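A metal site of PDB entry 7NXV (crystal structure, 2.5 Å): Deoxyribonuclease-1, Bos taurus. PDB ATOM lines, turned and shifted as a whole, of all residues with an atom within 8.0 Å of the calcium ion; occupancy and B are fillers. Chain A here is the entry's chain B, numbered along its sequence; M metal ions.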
ATOM      1  N   ALA A 200     -30.263  -9.921   8.403  1.00  0.00           N
ATOM      2  CA  ALA A 200     -28.941 -10.602   8.357  1.00  0.00           C
ATOM      3  C   ALA A 200     -28.048 -10.091   9.493  1.00  0.00           C
ATOM      4  O   ALA A 200     -28.195  -8.923   9.892  1.00  0.00           O
ATOM      5  CB  ALA A 200     -28.285 -10.387   7.011  1.00  0.00           C
ATOM      6  N   ASP A 201     -27.166 -10.959  10.001  1.00  0.00           N
ATOM      7  CA  ASP A 201     -26.130 -10.648  11.025  1.00  0.00           C
ATOM      8  C   ASP A 201     -24.749 -10.790  10.373  1.00  0.00           C
ATOM      9  O   ASP A 201     -24.373 -11.927  10.045  1.00  0.00           O
ATOM     10  CB  ASP A 201     -26.277 -11.564  12.236  1.00  0.00           C
ATOM     11  CG  ASP A 201     -25.288 -11.284  13.357  1.00  0.00           C
ATOM     12  OD1 ASP A 201     -24.820 -10.134  13.452  1.00  0.00           O
ATOM     13  OD2 ASP A 201     -25.001 -12.220  14.123  1.00  0.00           O
ATOM     14  N   THR A 202     -24.049  -9.658  10.184  1.00  0.00           N
ATOM     15  CA  THR A 202     -22.721  -9.582   9.523  1.00  0.00           C
ATOM     16  C   THR A 202     -21.630  -9.229  10.544  1.00  0.00           C
ATOM     17  O   THR A 202     -20.527  -8.846  10.095  1.00  0.00           O
ATOM     18  CB  THR A 202     -22.734  -8.582   8.361  1.00  0.00           C
ATOM     19  OG1 THR A 202     -22.857  -7.264   8.899  1.00  0.00           O
ATOM     20  CG2 THR A 202     -23.845  -8.849   7.372  1.00  0.00           C
ATOM     21  N   THR A 203     -21.924  -9.348  11.845  1.00  0.00           N
ATOM     22  CA  THR A 203     -20.964  -9.078  12.959  1.00  0.00           C
ATOM     23  C   THR A 203     -20.514 -10.406  13.561  1.00  0.00           C
ATOM     24  O   THR A 203     -21.374 -11.270  13.821  1.00  0.00           O
ATOM     25  CB  THR A 203     -21.576  -8.149  14.014  1.00  0.00           C
ATOM     26  OG1 THR A 203     -22.655  -8.833  14.662  1.00  0.00           O
ATOM     27  CG2 THR A 203     -22.073  -6.843  13.438  1.00  0.00           C
ATOM     28  N   ALA A 204     -19.199 -10.561  13.777  1.00  0.00           N
ATOM     29  CA  ALA A 204     -18.566 -11.721  14.454  1.00  0.00           C
ATOM     30  C   ALA A 204     -18.776 -11.599  15.968  1.00  0.00           C
ATOM     31  O   ALA A 204     -18.720 -12.636  16.654  1.00  0.00           O
ATOM     32  CB  ALA A 204     -17.102 -11.782  14.102  1.00  0.00           C
ATOM     33  N   THR A 205     -19.009 -10.374  16.468  1.00  0.00           N
ATOM     34  CA  THR A 205     -19.348 -10.083  17.890  1.00  0.00           C
ATOM     35  C   THR A 205     -20.769 -10.603  18.179  1.00  0.00           C
ATOM     36  O   THR A 205     -21.395 -11.161  17.253  1.00  0.00           O
ATOM     37  CB  THR A 205     -19.220  -8.589  18.210  1.00  0.00           C
ATOM     38  OG1 THR A 205     -20.155  -7.888  17.384  1.00  0.00           O
ATOM     39  CG2 THR A 205     -17.821  -8.051  17.995  1.00  0.00           C
ATOM     40  N   SER A 206     -21.249 -10.404  19.407  1.00  0.00           N
ATOM     41  CA  SER A 206     -22.562 -10.895  19.897  1.00  0.00           C
ATOM     42  C   SER A 206     -23.696  -9.923  19.491  1.00  0.00           C
ATOM     43  O   SER A 206     -24.858 -10.239  19.807  1.00  0.00           O
ATOM     44  CB  SER A 206     -22.533 -11.115  21.380  1.00  0.00           C
ATOM     45  OG  SER A 206     -22.064  -9.956  22.053  1.00  0.00           O
ATOM     46  N   THR A 207     -23.368  -8.809  18.815  1.00  0.00           N
ATOM     47  CA  THR A 207     -24.361  -7.853  18.255  1.00  0.00           C
ATOM     48  C   THR A 207     -25.107  -8.516  17.084  1.00  0.00           C
ATOM     49  O   THR A 207     -24.577  -9.508  16.529  1.00  0.00           O
ATOM     50  CB  THR A 207     -23.721  -6.549  17.774  1.00  0.00           C
ATOM     51  OG1 THR A 207     -22.605  -6.847  16.930  1.00  0.00           O
ATOM     52  CG2 THR A 207     -23.272  -5.658  18.921  1.00  0.00           C
ATOM     53  N   ASN A 208     -26.274  -7.977  16.734  1.00  0.00           N
ATOM     54  CA  ASN A 208     -27.104  -8.422  15.576  1.00  0.00           C
ATOM     55  C   ASN A 208     -27.372  -7.202  14.679  1.00  0.00           C
ATOM     56  O   ASN A 208     -28.419  -6.549  14.847  1.00  0.00           O
ATOM     57  CB  ASN A 208     -28.386  -9.100  16.050  1.00  0.00           C
ATOM     58  CG  ASN A 208     -29.249  -9.614  14.905  1.00  0.00           C
ATOM     59  OD1 ASN A 208     -28.770  -9.798  13.793  1.00  0.00           O
ATOM     60  ND2 ASN A 208     -30.509  -9.857  15.182  1.00  0.00           N
ATOM     61  N   CYS A 209     -26.430  -6.917  13.772  1.00  0.00           N
ATOM     62  CA  CYS A 209     -26.451  -5.747  12.859  1.00  0.00           C
ATOM     63  C   CYS A 209     -26.126  -6.189  11.426  1.00  0.00           C
ATOM     64  O   CYS A 209     -25.088  -6.848  11.237  1.00  0.00           O
ATOM     65  CB  CYS A 209     -25.440  -4.687  13.297  1.00  0.00           C
ATOM     66  SG  CYS A 209     -25.684  -4.060  14.986  1.00  0.00           S
ATOM     67  N   ASP A 234     -20.385 -16.961   8.135  1.00  0.00           N
ATOM     68  CA  ASP A 234     -19.989 -17.140   9.553  1.00  0.00           C
ATOM     69  C   ASP A 234     -18.761 -18.058   9.607  1.00  0.00           C
ATOM     70  O   ASP A 234     -18.946 -19.297   9.668  1.00  0.00           O
ATOM     71  CB  ASP A 234     -21.155 -17.671  10.391  1.00  0.00           C
ATOM     72  CG  ASP A 234     -20.875 -17.701  11.886  1.00  0.00           C
ATOM     73  OD1 ASP A 234     -19.687 -17.602  12.263  1.00  0.00           O
ATOM     74  OD2 ASP A 234     -21.846 -17.815  12.658  1.00  0.00           O
ATOM     75  N   GLN A 236     -16.621 -18.418  12.007  1.00  0.00           N
ATOM     76  CA  GLN A 236     -16.545 -19.061  13.353  1.00  0.00           C
ATOM     77  C   GLN A 236     -17.209 -20.442  13.270  1.00  0.00           C
ATOM     78  O   GLN A 236     -16.576 -21.427  13.696  1.00  0.00           O
ATOM     79  CB  GLN A 236     -17.208 -18.221  14.448  1.00  0.00           C
ATOM     80  CG  GLN A 236     -17.189 -18.900  15.805  1.00  0.00           C
ATOM     81  CD  GLN A 236     -17.683 -18.031  16.929  1.00  0.00           C
ATOM     82  OE1 GLN A 236     -18.003 -16.862  16.754  1.00  0.00           O
ATOM     83  NE2 GLN A 236     -17.746 -18.606  18.122  1.00  0.00           N
ATOM     84  N   ASN A 243     -15.010 -18.093  19.905  1.00  0.00           N
ATOM     85  CA  ASN A 243     -15.466 -16.702  19.659  1.00  0.00           C
ATOM     86  C   ASN A 243     -14.251 -15.762  19.738  1.00  0.00           C
ATOM     87  O   ASN A 243     -14.253 -14.755  19.004  1.00  0.00           O
ATOM     88  CB  ASN A 243     -16.575 -16.284  20.639  1.00  0.00           C
ATOM     89  CG  ASN A 243     -17.299 -15.020  20.205  1.00  0.00           C
ATOM     90  OD1 ASN A 243     -17.228 -13.998  20.875  1.00  0.00           O
ATOM     91  ND2 ASN A 243     -17.990 -15.080  19.076  1.00  0.00           N
ATOM     92  N   ASP A 251     -14.140  -8.642  13.397  1.00  0.00           N
ATOM     93  CA  ASP A 251     -15.416  -8.442  14.140  1.00  0.00           C
ATOM     94  C   ASP A 251     -16.595  -8.372  13.149  1.00  0.00           C
ATOM     95  O   ASP A 251     -17.740  -8.275  13.615  1.00  0.00           O
ATOM     96  CB  ASP A 251     -15.357  -7.217  15.070  1.00  0.00           C
ATOM     97  CG  ASP A 251     -15.032  -5.895  14.397  1.00  0.00           C
ATOM     98  OD1 ASP A 251     -14.510  -5.916  13.275  1.00  0.00           O
ATOM     99  OD2 ASP A 251     -15.305  -4.855  15.025  1.00  0.00           O
ATOM    100  N   TYR A 253     -18.252 -10.517   9.628  1.00  0.00           N
ATOM    101  CA  TYR A 253     -18.273 -11.633   8.654  1.00  0.00           C
ATOM    102  C   TYR A 253     -18.151 -11.054   7.247  1.00  0.00           C
ATOM    103  O   TYR A 253     -18.549  -9.910   7.021  1.00  0.00           O
ATOM    104  CB  TYR A 253     -19.573 -12.440   8.757  1.00  0.00           C
ATOM    105  CG  TYR A 253     -19.838 -13.097  10.086  1.00  0.00           C
ATOM    106  CD1 TYR A 253     -18.822 -13.711  10.800  1.00  0.00           C
ATOM    107  CD2 TYR A 253     -21.119 -13.144  10.614  1.00  0.00           C
ATOM    108  CE1 TYR A 253     -19.062 -14.329  12.012  1.00  0.00           C
ATOM    109  CE2 TYR A 253     -21.380 -13.751  11.828  1.00  0.00           C
ATOM    110  CZ  TYR A 253     -20.346 -14.346  12.530  1.00  0.00           C
ATOM    111  OH  TYR A 253     -20.586 -14.963  13.727  1.00  0.00           O
HETATM  112 CA    CA M   1     -23.173 -11.236  15.564  1.00  0.00          CA
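OG1 of Thr 207 is in hydrogen-bond range of OG1 of Thr 205 (2.7 Å).
The calcium ion is bound by the backbone carbonyl oxygen (O) of Thr 207 (2.4 Å), the backbone carbonyl oxygen (O) of Thr 205 (2.5 Å), the backbone carbonyl oxygen (O) of Thr 203 (2.5 Å), the side-chain carboxylate (OD2) of Asp 201 (2.5 Å), the side-chain hydroxyl (OG1) of Thr 203 (2.6 Å) and the side-chain carboxylate (OD1) of Asp 201 (2.9 Å).
The calcium ion has six donor atoms within binding distance.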
